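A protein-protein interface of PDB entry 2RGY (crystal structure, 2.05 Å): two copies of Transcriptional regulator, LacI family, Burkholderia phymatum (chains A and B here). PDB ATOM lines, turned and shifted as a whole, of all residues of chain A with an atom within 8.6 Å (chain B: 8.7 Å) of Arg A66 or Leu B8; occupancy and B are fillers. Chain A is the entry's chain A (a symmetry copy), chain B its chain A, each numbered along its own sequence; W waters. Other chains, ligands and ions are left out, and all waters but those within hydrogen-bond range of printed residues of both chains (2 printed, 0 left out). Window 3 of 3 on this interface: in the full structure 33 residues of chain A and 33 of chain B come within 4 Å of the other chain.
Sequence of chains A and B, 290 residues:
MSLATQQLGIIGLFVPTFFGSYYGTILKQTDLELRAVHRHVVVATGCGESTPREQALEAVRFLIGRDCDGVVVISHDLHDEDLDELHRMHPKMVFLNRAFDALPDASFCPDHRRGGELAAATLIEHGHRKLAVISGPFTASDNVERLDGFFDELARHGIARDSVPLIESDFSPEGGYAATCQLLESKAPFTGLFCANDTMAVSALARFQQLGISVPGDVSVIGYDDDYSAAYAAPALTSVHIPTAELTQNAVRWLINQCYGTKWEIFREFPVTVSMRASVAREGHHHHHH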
ATOM      1  N   LEU A   8      16.442 -21.210  13.801  1.00  0.00           N
ATOM      2  CA  LEU A   8      17.644 -21.988  13.367  1.00  0.00           C
ATOM      3  C   LEU A   8      18.786 -21.063  12.963  1.00  0.00           C
ATOM      4  O   LEU A   8      19.951 -21.449  13.009  1.00  0.00           O
ATOM      5  CB  LEU A   8      17.280 -22.903  12.190  1.00  0.00           C
ATOM      6  CG  LEU A   8      18.363 -23.752  11.516  1.00  0.00           C
ATOM      7  CD1 LEU A   8      18.988 -24.731  12.512  1.00  0.00           C
ATOM      8  CD2 LEU A   8      17.716 -24.521  10.363  1.00  0.00           C
ATOM      9  N   GLY A   9      18.449 -19.842  12.567  1.00  0.00           N
ATOM     10  CA  GLY A   9      19.466 -18.889  12.158  1.00  0.00           C
ATOM     11  C   GLY A   9      19.998 -19.142  10.755  1.00  0.00           C
ATOM     12  O   GLY A   9      21.096 -18.699  10.412  1.00  0.00           O
ATOM     13  N   ILE A  10      19.220 -19.862   9.949  1.00  0.00           N
ATOM     14  CA  ILE A  10      19.609 -20.179   8.575  1.00  0.00           C
ATOM     15  C   ILE A  10      18.474 -19.917   7.598  1.00  0.00           C
ATOM     16  O   ILE A  10      17.313 -20.232   7.869  1.00  0.00           O
ATOM     17  CB  ILE A  10      19.978 -21.675   8.386  1.00  0.00           C
ATOM     18  CG1 ILE A  10      20.826 -22.184   9.547  1.00  0.00           C
ATOM     19  CG2 ILE A  10      20.727 -21.858   7.084  1.00  0.00           C
ATOM     20  CD1 ILE A  10      22.048 -21.374   9.822  1.00  0.00           C
ATOM     21  N   GLY A  12      17.281 -20.677   3.655  1.00  0.00           N
ATOM     22  CA  GLY A  12      17.612 -21.577   2.566  1.00  0.00           C
ATOM     23  C   GLY A  12      17.579 -20.857   1.235  1.00  0.00           C
ATOM     24  O   GLY A  12      16.830 -19.900   1.080  1.00  0.00           O
ATOM     25  N   HIS A  40      23.564 -17.651   8.618  1.00  0.00           N
ATOM     26  CA  HIS A  40      24.050 -18.428   7.485  1.00  0.00           C
ATOM     27  C   HIS A  40      23.061 -18.778   6.373  1.00  0.00           C
ATOM     28  O   HIS A  40      21.848 -18.635   6.511  1.00  0.00           O
ATOM     29  CB  HIS A  40      24.666 -19.727   7.996  1.00  0.00           C
ATOM     30  CG  HIS A  40      25.696 -19.538   9.066  1.00  0.00           C
ATOM     31  ND1 HIS A  40      25.378 -19.156  10.353  1.00  0.00           N
ATOM     32  CD2 HIS A  40      27.035 -19.725   9.050  1.00  0.00           C
ATOM     33  CE1 HIS A  40      26.477 -19.123  11.084  1.00  0.00           C
ATOM     34  NE2 HIS A  40      27.497 -19.464  10.319  1.00  0.00           N
ATOM     35  N   VAL A  42      22.062 -21.867   3.527  1.00  0.00           N
ATOM     36  CA  VAL A  42      22.199 -23.235   3.076  1.00  0.00           C
ATOM     37  C   VAL A  42      21.762 -23.166   1.622  1.00  0.00           C
ATOM     38  O   VAL A  42      20.684 -22.650   1.323  1.00  0.00           O
ATOM     39  CB  VAL A  42      21.264 -24.187   3.838  1.00  0.00           C
ATOM     40  CG1 VAL A  42      21.105 -25.490   3.058  1.00  0.00           C
ATOM     41  CG2 VAL A  42      21.842 -24.475   5.214  1.00  0.00           C
ATOM     42  N   ALA A  59      14.261 -30.108  -4.348  1.00  0.00           N
ATOM     43  CA  ALA A  59      15.273 -29.309  -3.670  1.00  0.00           C
ATOM     44  C   ALA A  59      14.649 -28.323  -2.687  1.00  0.00           C
ATOM     45  O   ALA A  59      15.103 -28.204  -1.549  1.00  0.00           O
ATOM     46  CB  ALA A  59      16.114 -28.573  -4.685  1.00  0.00           C
ATOM     47  N   VAL A  60      13.611 -27.612  -3.116  1.00  0.00           N
ATOM     48  CA  VAL A  60      12.958 -26.659  -2.223  1.00  0.00           C
ATOM     49  C   VAL A  60      12.307 -27.387  -1.044  1.00  0.00           C
ATOM     50  O   VAL A  60      12.372 -26.913   0.089  1.00  0.00           O
ATOM     51  CB  VAL A  60      11.901 -25.811  -2.962  1.00  0.00           C
ATOM     52  CG1 VAL A  60      11.237 -24.851  -1.989  1.00  0.00           C
ATOM     53  CG2 VAL A  60      12.564 -25.031  -4.093  1.00  0.00           C
ATOM     54  N   ARG A  61      11.686 -28.537  -1.296  1.00  0.00           N
ATOM     55  CA  ARG A  61      11.078 -29.295  -0.203  1.00  0.00           C
ATOM     56  C   ARG A  61      12.148 -29.775   0.782  1.00  0.00           C
ATOM     57  O   ARG A  61      11.890 -29.912   1.973  1.00  0.00           O
ATOM     58  CB  ARG A  61      10.273 -30.482  -0.755  1.00  0.00           C
ATOM     59  CG  ARG A  61       8.945 -30.062  -1.392  1.00  0.00           C
ATOM     60  CD  ARG A  61       8.086 -31.251  -1.852  1.00  0.00           C
ATOM     61  NE  ARG A  61       8.697 -31.993  -2.954  1.00  0.00           N
ATOM     62  CZ  ARG A  61       8.066 -32.347  -4.077  1.00  0.00           C
ATOM     63  NH1 ARG A  61       6.787 -32.032  -4.273  1.00  0.00           N
ATOM     64  NH2 ARG A  61       8.717 -33.028  -5.008  1.00  0.00           N
ATOM     65  N   PHE A  62      13.352 -30.011   0.272  1.00  0.00           N
ATOM     66  CA  PHE A  62      14.490 -30.453   1.075  1.00  0.00           C
ATOM     67  C   PHE A  62      14.954 -29.316   1.997  1.00  0.00           C
ATOM     68  O   PHE A  62      15.412 -29.554   3.111  1.00  0.00           O
ATOM     69  CB  PHE A  62      15.635 -30.866   0.144  1.00  0.00           C
ATOM     70  CG  PHE A  62      16.839 -31.421   0.852  1.00  0.00           C
ATOM     71  CD1 PHE A  62      16.716 -32.516   1.706  1.00  0.00           C
ATOM     72  CD2 PHE A  62      18.114 -30.875   0.628  1.00  0.00           C
ATOM     73  CE1 PHE A  62      17.842 -33.076   2.334  1.00  0.00           C
ATOM     74  CE2 PHE A  62      19.253 -31.423   1.246  1.00  0.00           C
ATOM     75  CZ  PHE A  62      19.116 -32.531   2.107  1.00  0.00           C
ATOM     76  N   LEU A  63      14.843 -28.080   1.517  1.00  0.00           N
ATOM     77  CA  LEU A  63      15.227 -26.915   2.307  1.00  0.00           C
ATOM     78  C   LEU A  63      14.174 -26.690   3.386  1.00  0.00           C
ATOM     79  O   LEU A  63      14.493 -26.426   4.548  1.00  0.00           O
ATOM     80  CB  LEU A  63      15.319 -25.667   1.417  1.00  0.00           C
ATOM     81  CG  LEU A  63      16.469 -25.586   0.405  1.00  0.00           C
ATOM     82  CD1 LEU A  63      16.290 -24.350  -0.472  1.00  0.00           C
ATOM     83  CD2 LEU A  63      17.807 -25.538   1.135  1.00  0.00           C
ATOM     84  N   ILE A  64      12.910 -26.792   2.985  1.00  0.00           N
ATOM     85  CA  ILE A  64      11.787 -26.604   3.900  1.00  0.00           C
ATOM     86  C   ILE A  64      11.822 -27.664   4.992  1.00  0.00           C
ATOM     87  O   ILE A  64      11.500 -27.397   6.143  1.00  0.00           O
ATOM     88  CB  ILE A  64      10.432 -26.699   3.148  1.00  0.00           C
ATOM     89  CG1 ILE A  64      10.275 -25.518   2.196  1.00  0.00           C
ATOM     90  CG2 ILE A  64       9.276 -26.713   4.141  1.00  0.00           C
ATOM     91  CD1 ILE A  64       8.979 -25.526   1.429  1.00  0.00           C
ATOM     92  N   GLY A  65      12.224 -28.876   4.621  1.00  0.00           N
ATOM     93  CA  GLY A  65      12.291 -29.955   5.589  1.00  0.00           C
ATOM     94  C   GLY A  65      13.332 -29.718   6.669  1.00  0.00           C
ATOM     95  O   GLY A  65      13.193 -30.221   7.780  1.00  0.00           O
ATOM     96  N   ARG A  66      14.375 -28.956   6.352  1.00  0.00           N
ATOM     97  CA  ARG A  66      15.431 -28.664   7.321  1.00  0.00           C
ATOM     98  C   ARG A  66      15.024 -27.545   8.278  1.00  0.00           C
ATOM     99  O   ARG A  66      15.762 -27.199   9.199  1.00  0.00           O
ATOM    100  CB  ARG A  66      16.724 -28.258   6.605  1.00  0.00           C
ATOM    101  CG  ARG A  66      17.936 -28.146   7.540  1.00  0.00           C
ATOM    102  CD  ARG A  66      18.181 -29.462   8.267  1.00  0.00           C
ATOM    103  NE  ARG A  66      19.147 -29.371   9.363  1.00  0.00           N
ATOM    104  CZ  ARG A  66      18.901 -28.800  10.536  1.00  0.00           C
ATOM    105  NH1 ARG A  66      17.725 -28.254  10.777  1.00  0.00           N
ATOM    106  NH2 ARG A  66      19.821 -28.806  11.483  1.00  0.00           N
ATOM    107  N   ASP A  67      13.838 -26.990   8.052  1.00  0.00           N
ATOM    108  CA  ASP A  67      13.311 -25.897   8.863  1.00  0.00           C
ATOM    109  C   ASP A  67      14.120 -24.612   8.778  1.00  0.00           C
ATOM    110  O   ASP A  67      14.436 -23.990   9.802  1.00  0.00           O
ATOM    111  CB  ASP A  67      13.172 -26.312  10.324  1.00  0.00           C
ATOM    112  CG  ASP A  67      11.946 -27.163  10.562  1.00  0.00           C
ATOM    113  OD1 ASP A  67      10.849 -26.734  10.144  1.00  0.00           O
ATOM    114  OD2 ASP A  67      12.084 -28.251  11.165  1.00  0.00           O
ATOM    115  N   CYS A  68      14.464 -24.220   7.556  1.00  0.00           N
ATOM    116  CA  CYS A  68      15.189 -22.972   7.361  1.00  0.00           C
ATOM    117  C   CYS A  68      14.200 -21.906   7.832  1.00  0.00           C
ATOM    118  O   CYS A  68      12.993 -22.085   7.673  1.00  0.00           O
ATOM    119  CB  CYS A  68      15.513 -22.779   5.882  1.00  0.00           C
ATOM    120  SG  CYS A  68      16.700 -23.967   5.215  1.00  0.00           S
ATOM    121  N   ASP A  69      14.685 -20.817   8.421  1.00  0.00           N
ATOM    122  CA  ASP A  69      13.778 -19.774   8.893  1.00  0.00           C
ATOM    123  C   ASP A  69      13.026 -19.136   7.726  1.00  0.00           C
ATOM    124  O   ASP A  69      11.877 -18.719   7.860  1.00  0.00           O
ATOM    125  CB  ASP A  69      14.546 -18.703   9.666  1.00  0.00           C
ATOM    126  CG  ASP A  69      15.236 -19.261  10.894  1.00  0.00           C
ATOM    127  OD1 ASP A  69      14.591 -20.040  11.628  1.00  0.00           O
ATOM    128  OD2 ASP A  69      16.411 -18.915  11.127  1.00  0.00           O
ATOM    129  N   VAL A  71      13.054 -19.084   3.039  1.00  0.00           N
ATOM    130  CA  VAL A  71      13.601 -19.699   1.843  1.00  0.00           C
ATOM    131  C   VAL A  71      13.559 -18.756   0.645  1.00  0.00           C
ATOM    132  O   VAL A  71      12.514 -18.169   0.339  1.00  0.00           O
ATOM    133  CB  VAL A  71      12.837 -20.988   1.484  1.00  0.00           C
ATOM    134  CG1 VAL A  71      13.466 -21.631   0.257  1.00  0.00           C
ATOM    135  CG2 VAL A  71      12.854 -21.945   2.660  1.00  0.00           C
ATOM    136  N   HIS A  90       5.562 -23.361   3.467  1.00  0.00           N
ATOM    137  CA  HIS A  90       6.459 -22.485   4.210  1.00  0.00           C
ATOM    138  C   HIS A  90       6.141 -21.048   3.814  1.00  0.00           C
ATOM    139  O   HIS A  90       6.634 -20.553   2.799  1.00  0.00           O
ATOM    140  CB  HIS A  90       7.907 -22.844   3.849  1.00  0.00           C
ATOM    141  CG  HIS A  90       8.925 -22.258   4.775  1.00  0.00           C
ATOM    142  ND1 HIS A  90       9.250 -20.917   4.774  1.00  0.00           N
ATOM    143  CD2 HIS A  90       9.675 -22.825   5.745  1.00  0.00           C
ATOM    144  CE1 HIS A  90      10.157 -20.685   5.706  1.00  0.00           C
ATOM    145  NE2 HIS A  90      10.434 -21.828   6.309  1.00  0.00           N
ATOM    146  N   LEU B   8      24.248 -31.818  13.731  1.00  0.00           N
ATOM    147  CA  LEU B   8      23.463 -30.727  13.075  1.00  0.00           C
ATOM    148  C   LEU B   8      23.009 -31.134  11.678  1.00  0.00           C
ATOM    149  O   LEU B   8      22.023 -30.613  11.163  1.00  0.00           O
ATOM    150  CB  LEU B   8      24.309 -29.450  12.991  1.00  0.00           C
ATOM    151  CG  LEU B   8      23.750 -28.206  12.293  1.00  0.00           C
ATOM    152  CD1 LEU B   8      22.478 -27.714  12.988  1.00  0.00           C
ATOM    153  CD2 LEU B   8      24.822 -27.116  12.332  1.00  0.00           C
ATOM    154  N   GLY B   9      23.731 -32.065  11.067  1.00  0.00           N
ATOM    155  CA  GLY B   9      23.381 -32.516   9.731  1.00  0.00           C
ATOM    156  C   GLY B   9      23.803 -31.544   8.639  1.00  0.00           C
ATOM    157  O   GLY B   9      23.258 -31.570   7.533  1.00  0.00           O
ATOM    158  N   ILE B  10      24.768 -30.683   8.954  1.00  0.00           N
ATOM    159  CA  ILE B  10      25.269 -29.696   7.999  1.00  0.00           C
ATOM    160  C   ILE B  10      26.790 -29.668   7.969  1.00  0.00           C
ATOM    161  O   ILE B  10      27.449 -29.730   9.009  1.00  0.00           O
ATOM    162  CB  ILE B  10      24.838 -28.247   8.351  1.00  0.00           C
ATOM    163  CG1 ILE B  10      23.378 -28.198   8.791  1.00  0.00           C
ATOM    164  CG2 ILE B  10      25.044 -27.345   7.155  1.00  0.00           C
ATOM    165  CD1 ILE B  10      22.420 -28.809   7.823  1.00  0.00           C
ATOM    166  N   ILE B  11      27.343 -29.570   6.771  1.00  0.00           N
ATOM    167  CA  ILE B  11      28.777 -29.466   6.615  1.00  0.00           C
ATOM    168  C   ILE B  11      29.003 -28.062   6.081  1.00  0.00           C
ATOM    169  O   ILE B  11      28.241 -27.584   5.247  1.00  0.00           O
ATOM    170  CB  ILE B  11      29.320 -30.537   5.637  1.00  0.00           C
ATOM    171  CG1 ILE B  11      29.438 -31.875   6.376  1.00  0.00           C
ATOM    172  CG2 ILE B  11      30.675 -30.115   5.075  1.00  0.00           C
ATOM    173  CD1 ILE B  11      30.065 -32.991   5.559  1.00  0.00           C
ATOM    174  N   GLY B  12      30.015 -27.377   6.594  1.00  0.00           N
ATOM    175  CA  GLY B  12      30.279 -26.028   6.126  1.00  0.00           C
ATOM    176  C   GLY B  12      31.261 -26.034   4.974  1.00  0.00           C
ATOM    177  O   GLY B  12      32.100 -26.923   4.895  1.00  0.00           O
ATOM    178  N   HIS B  38      21.333 -37.205   2.363  1.00  0.00           N
ATOM    179  CA  HIS B  38      20.227 -36.424   2.910  1.00  0.00           C
ATOM    180  C   HIS B  38      20.626 -35.333   3.897  1.00  0.00           C
ATOM    181  O   HIS B  38      19.940 -35.112   4.892  1.00  0.00           O
ATOM    182  CB  HIS B  38      19.221 -37.371   3.568  1.00  0.00           C
ATOM    183  CG  HIS B  38      18.791 -38.495   2.677  1.00  0.00           C
ATOM    184  ND1 HIS B  38      18.153 -38.286   1.473  1.00  0.00           N
ATOM    185  CD2 HIS B  38      18.935 -39.837   2.799  1.00  0.00           C
ATOM    186  CE1 HIS B  38      17.923 -39.450   0.890  1.00  0.00           C
ATOM    187  NE2 HIS B  38      18.387 -40.406   1.675  1.00  0.00           N
ATOM    188  N   ARG B  39      21.728 -34.647   3.613  1.00  0.00           N
ATOM    189  CA  ARG B  39      22.190 -33.576   4.479  1.00  0.00           C
ATOM    190  C   ARG B  39      22.467 -32.303   3.681  1.00  0.00           C
ATOM    191  O   ARG B  39      22.495 -32.333   2.454  1.00  0.00           O
ATOM    192  CB  ARG B  39      23.414 -34.037   5.270  1.00  0.00           C
ATOM    193  CG  ARG B  39      23.048 -35.114   6.300  1.00  0.00           C
ATOM    194  CD  ARG B  39      24.255 -35.644   7.050  1.00  0.00           C
ATOM    195  NE  ARG B  39      23.899 -36.558   8.140  1.00  0.00           N
ATOM    196  CZ  ARG B  39      23.684 -37.866   8.003  1.00  0.00           C
ATOM    197  NH1 ARG B  39      23.774 -38.450   6.814  1.00  0.00           N
ATOM    198  NH2 ARG B  39      23.417 -38.603   9.071  1.00  0.00           N
ATOM    199  N   HIS B  40      22.680 -31.194   4.381  1.00  0.00           N
ATOM    200  CA  HIS B  40      22.876 -29.904   3.732  1.00  0.00           C
ATOM    201  C   HIS B  40      24.259 -29.257   3.814  1.00  0.00           C
ATOM    202  O   HIS B  40      25.124 -29.664   4.588  1.00  0.00           O
ATOM    203  CB  HIS B  40      21.856 -28.910   4.278  1.00  0.00           C
ATOM    204  CG  HIS B  40      20.439 -29.390   4.220  1.00  0.00           C
ATOM    205  ND1 HIS B  40      19.950 -30.381   5.046  1.00  0.00           N
ATOM    206  CD2 HIS B  40      19.395 -28.981   3.464  1.00  0.00           C
ATOM    207  CE1 HIS B  40      18.663 -30.555   4.806  1.00  0.00           C
ATOM    208  NE2 HIS B  40      18.301 -29.719   3.851  1.00  0.00           N
ATOM    209  N   VAL B  41      24.442 -28.222   3.009  1.00  0.00           N
ATOM    210  CA  VAL B  41      25.696 -27.500   2.983  1.00  0.00           C
ATOM    211  C   VAL B  41      25.451 -26.011   3.205  1.00  0.00           C
ATOM    212  O   VAL B  41      24.553 -25.414   2.610  1.00  0.00           O
ATOM    213  CB  VAL B  41      26.407 -27.682   1.636  1.00  0.00           C
ATOM    214  CG1 VAL B  41      25.513 -27.184   0.523  1.00  0.00           C
ATOM    215  CG2 VAL B  41      27.731 -26.939   1.629  1.00  0.00           C
ATOM    216  N   VAL B  42      26.237 -25.431   4.097  1.00  0.00           N
ATOM    217  CA  VAL B  42      26.169 -24.012   4.369  1.00  0.00           C
ATOM    218  C   VAL B  42      27.418 -23.469   3.697  1.00  0.00           C
ATOM    219  O   VAL B  42      28.518 -23.968   3.939  1.00  0.00           O
ATOM    220  CB  VAL B  42      26.237 -23.712   5.875  1.00  0.00           C
ATOM    221  CG1 VAL B  42      26.610 -22.248   6.096  1.00  0.00           C
ATOM    222  CG2 VAL B  42      24.889 -24.005   6.514  1.00  0.00           C
ATOM    223  N   LEU B  63      31.877 -20.407  10.237  1.00  0.00           N
ATOM    224  CA  LEU B  63      31.302 -21.716   9.948  1.00  0.00           C
ATOM    225  C   LEU B  63      31.474 -22.605  11.175  1.00  0.00           C
ATOM    226  O   LEU B  63      30.555 -23.321  11.582  1.00  0.00           O
ATOM    227  CB  LEU B  63      32.009 -22.362   8.748  1.00  0.00           C
ATOM    228  CG  LEU B  63      31.777 -21.753   7.359  1.00  0.00           C
ATOM    229  CD1 LEU B  63      32.679 -22.443   6.342  1.00  0.00           C
ATOM    230  CD2 LEU B  63      30.311 -21.897   6.963  1.00  0.00           C
ATOM    231  N   ILE B  64      32.668 -22.555  11.757  1.00  0.00           N
ATOM    232  CA  ILE B  64      32.989 -23.348  12.942  1.00  0.00           C
ATOM    233  C   ILE B  64      32.093 -22.936  14.102  1.00  0.00           C
ATOM    234  O   ILE B  64      31.670 -23.764  14.899  1.00  0.00           O
ATOM    235  CB  ILE B  64      34.473 -23.156  13.357  1.00  0.00           C
ATOM    236  CG1 ILE B  64      35.396 -23.760  12.304  1.00  0.00           C
ATOM    237  CG2 ILE B  64      34.734 -23.816  14.706  1.00  0.00           C
ATOM    238  CD1 ILE B  64      36.860 -23.625  12.633  1.00  0.00           C
ATOM    239  N   GLY B  65      31.801 -21.642  14.186  1.00  0.00           N
ATOM    240  CA  GLY B  65      30.954 -21.151  15.258  1.00  0.00           C
ATOM    241  C   GLY B  65      29.531 -21.675  15.177  1.00  0.00           C
ATOM    242  O   GLY B  65      28.856 -21.785  16.196  1.00  0.00           O
ATOM    243  N   ARG B  66      29.070 -21.999  13.972  1.00  0.00           N
ATOM    244  CA  ARG B  66      27.715 -22.516  13.786  1.00  0.00           C
ATOM    245  C   ARG B  66      27.630 -24.005  14.116  1.00  0.00           C
ATOM    246  O   ARG B  66      26.557 -24.604  14.072  1.00  0.00           O
ATOM    247  CB  ARG B  66      27.247 -22.301  12.342  1.00  0.00           C
ATOM    248  CG  ARG B  66      25.762 -22.618  12.123  1.00  0.00           C
ATOM    249  CD  ARG B  66      24.887 -21.776  13.044  1.00  0.00           C
ATOM    250  NE  ARG B  66      23.485 -22.196  13.087  1.00  0.00           N
ATOM    251  CZ  ARG B  66      23.045 -23.284  13.708  1.00  0.00           C
ATOM    252  NH1 ARG B  66      23.890 -24.079  14.336  1.00  0.00           N
ATOM    253  NH2 ARG B  66      21.754 -23.557  13.733  1.00  0.00           N
ATOM    254  N   ASP B  67      28.773 -24.592  14.451  1.00  0.00           N
ATOM    255  CA  ASP B  67      28.867 -26.012  14.775  1.00  0.00           C
ATOM    256  C   ASP B  67      28.533 -26.938  13.617  1.00  0.00           C
ATOM    257  O   ASP B  67      27.767 -27.900  13.771  1.00  0.00           O
ATOM    258  CB  ASP B  67      27.990 -26.362  15.973  1.00  0.00           C
ATOM    259  CG  ASP B  67      28.624 -25.957  17.284  1.00  0.00           C
ATOM    260  OD1 ASP B  67      29.797 -26.329  17.503  1.00  0.00           O
ATOM    261  OD2 ASP B  67      27.949 -25.274  18.086  1.00  0.00           O
ATOM    262  N   CYS B  68      29.102 -26.643  12.453  1.00  0.00           N
ATOM    263  CA  CYS B  68      28.893 -27.503  11.294  1.00  0.00           C
ATOM    264  C   CYS B  68      29.545 -28.822  11.706  1.00  0.00           C
ATOM    265  O   CYS B  68      30.532 -28.810  12.441  1.00  0.00           O
ATOM    266  CB  CYS B  68      29.601 -26.918  10.075  1.00  0.00           C
ATOM    267  SG  CYS B  68      28.898 -25.365   9.475  1.00  0.00           S
ATOM    268  N   ASP B  69      29.004 -29.953  11.263  1.00  0.00           N
ATOM    269  CA  ASP B  69      29.589 -31.239  11.635  1.00  0.00           C
ATOM    270  C   ASP B  69      31.002 -31.379  11.072  1.00  0.00           C
ATOM    271  O   ASP B  69      31.869 -32.008  11.676  1.00  0.00           O
ATOM    272  CB  ASP B  69      28.714 -32.391  11.140  1.00  0.00           C
ATOM    273  CG  ASP B  69      27.325 -32.360  11.743  1.00  0.00           C
ATOM    274  OD1 ASP B  69      27.220 -32.145  12.970  1.00  0.00           O
ATOM    275  OD2 ASP B  69      26.346 -32.558  10.996  1.00  0.00           O
ATOM    276  N   GLY B  70      31.217 -30.790   9.905  1.00  0.00           N
ATOM    277  CA  GLY B  70      32.518 -30.834   9.263  1.00  0.00           C
ATOM    278  C   GLY B  70      32.675 -29.580   8.429  1.00  0.00           C
ATOM    279  O   GLY B  70      31.682 -28.935   8.095  1.00  0.00           O
ATOM    280  N   CYS B 259      32.442 -37.852   9.605  1.00  0.00           N
ATOM    281  CA  CYS B 259      31.296 -37.196  10.230  1.00  0.00           C
ATOM    282  C   CYS B 259      30.031 -38.011  10.415  1.00  0.00           C
ATOM    283  O   CYS B 259      29.429 -37.990  11.494  1.00  0.00           O
ATOM    284  CB  CYS B 259      30.892 -35.952   9.440  1.00  0.00           C
ATOM    285  SG  CYS B 259      31.991 -34.551   9.539  1.00  0.00           S
ATOM    286  N   TYR B 260      29.623 -38.719   9.365  1.00  0.00           N
ATOM    287  CA  TYR B 260      28.379 -39.464   9.420  1.00  0.00           C
ATOM    288  C   TYR B 260      28.404 -40.984   9.341  1.00  0.00           C
ATOM    289  O   TYR B 260      27.348 -41.605   9.211  1.00  0.00           O
ATOM    290  CB  TYR B 260      27.437 -38.911   8.354  1.00  0.00           C
ATOM    291  CG  TYR B 260      27.314 -37.399   8.390  1.00  0.00           C
ATOM    292  CD1 TYR B 260      26.827 -36.750   9.518  1.00  0.00           C
ATOM    293  CD2 TYR B 260      27.662 -36.621   7.286  1.00  0.00           C
ATOM    294  CE1 TYR B 260      26.682 -35.365   9.550  1.00  0.00           C
ATOM    295  CE2 TYR B 260      27.519 -35.235   7.308  1.00  0.00           C
ATOM    296  CZ  TYR B 260      27.027 -34.612   8.443  1.00  0.00           C
ATOM    297  OH  TYR B 260      26.856 -33.244   8.473  1.00  0.00           O
HETATM  298  O   HOH W   1      20.647 -31.548   7.519  1.00  0.00           O
HETATM  299  O   HOH W   2      23.099 -19.180  12.017  1.00  0.00           O
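O of Leu B8 lies within hydrogen-bond range of NH2 of Arg A66, 2.9 Å away.
NE2 of His B40 is in hydrogen-bond range of O of Phe A62.
NH2 of Arg B66 lies within hydrogen-bond range of O of Leu A8 (2.9 Å).
The backbone NH of Leu A8 lies within hydrogen-bond range of the side-chain carboxylate of Asp A69 (3.1 Å).
The backbone carbonyl oxygen of Ile B10 is in hydrogen-bond range of the backbone NH of Asp B69 (2.7 Å).
The backbone NH (N) of Leu B8 sits at hydrogen-bond distance from the side-chain carboxylate (OD1) of Asp B69 (3.1 Å).
O of Ile A10 lies within hydrogen-bond range of N of Asp A69 (2.7 Å).
The backbone NH (N) of Val B42 is in hydrogen-bond range of the backbone carbonyl oxygen (O) of Ile B11, at 3.2 Å.
O of Gly B9 sits at hydrogen-bond distance from N of His B40 (3.2 Å).
CD1 of Ile A10 touches NE of Arg B66, at 3.7 Å.
CB of His A40 touches CG1 of Val B42, at 3.7 Å.
NE2 of His A40 touches CB of Arg B66, 3.5 Å away.
CG1 of Val A42 touches CB of His B40, 3.7 Å away.
Val B41 touches Val A42.
CG2 of Val A42 touches CG2 of Val B42 (3.3 Å).
Phe A62 touches His B38 (CZ to C, 3.7 Å).
Phe A62 touches Arg B39.
Arg A66 touches Ile B10.
His B40 touches Arg A66.
Printed residues of chain B within 4 Å of Leu A8: Arg B66 (2.9 Å).
Of the printed residues of chain B, Val A42 touches His B40, Val B41 and Val B42.
Arg A61 touches none of the printed residues of chain B.
No residue of chain B comes within 4 Å of Gly A65.
Of chain B, only Leu B8 (2.9 Å), Ile B10 (3.7 Å) and His B40 (3.5 Å) come within 4 Å of Arg A66.
His A90 touches none of the printed residues of chain B.
Of chain A, only Arg A66 (2.9 Å) comes within 4 Å of Leu B8.
Of the printed residues of chain A, Arg B66 touches Leu A8 (2.9 Å), Ile A10 (3.7 Å) and His A40 (3.5 Å).
The nearest residue of chain A that does not touch Leu B8 is Leu A8 (4.6 Å).
Of the 19 printed residues of chain A, 6 touch a printed residue of chain B.
Hydrophobic or aromatic side chains of chain A that line the printed part of chain B: Leu A8, Ile A10, His A40, Val A42 and Phe A62.
Hydrophobic or aromatic side chains of chain B within 4 Å of the printed part of chain A: Leu B8, Ile B10, His B40 and Val B42.
Among the printed residues, 13 pairs touch across the chains.
Leu A8 touches Arg B66, and with the chains exchanged Arg A66 touches Leu B8.
Ile A10 touches Arg B66, and with the chains exchanged Arg A66 touches Ile B10.
His A40 touches Arg B66, and with the chains exchanged Arg A66 touches His B40.
Val A42 touches its own counterpart, Val B42.
Positions printed for both chains: 8, 9, 10, 12, 40, 42, 63, 64, 65, 66, 67, 68 and 69.
Of the 13 pairs that touch across the chains among the printed residues, 9 have their exchanged pair printed and touching as well.
Water W2 lies within hydrogen-bond range of the backbone carbonyl oxygen of Gly A9, a ring nitrogen (ND1) of His A40 and the guanidinium group of Arg B66.
Water W1 lies within hydrogen-bond range of O of Gly B9 (2.6 Å), ND1 of His B40 (2.8 Å) and NE of Arg A66 (3.2 Å).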
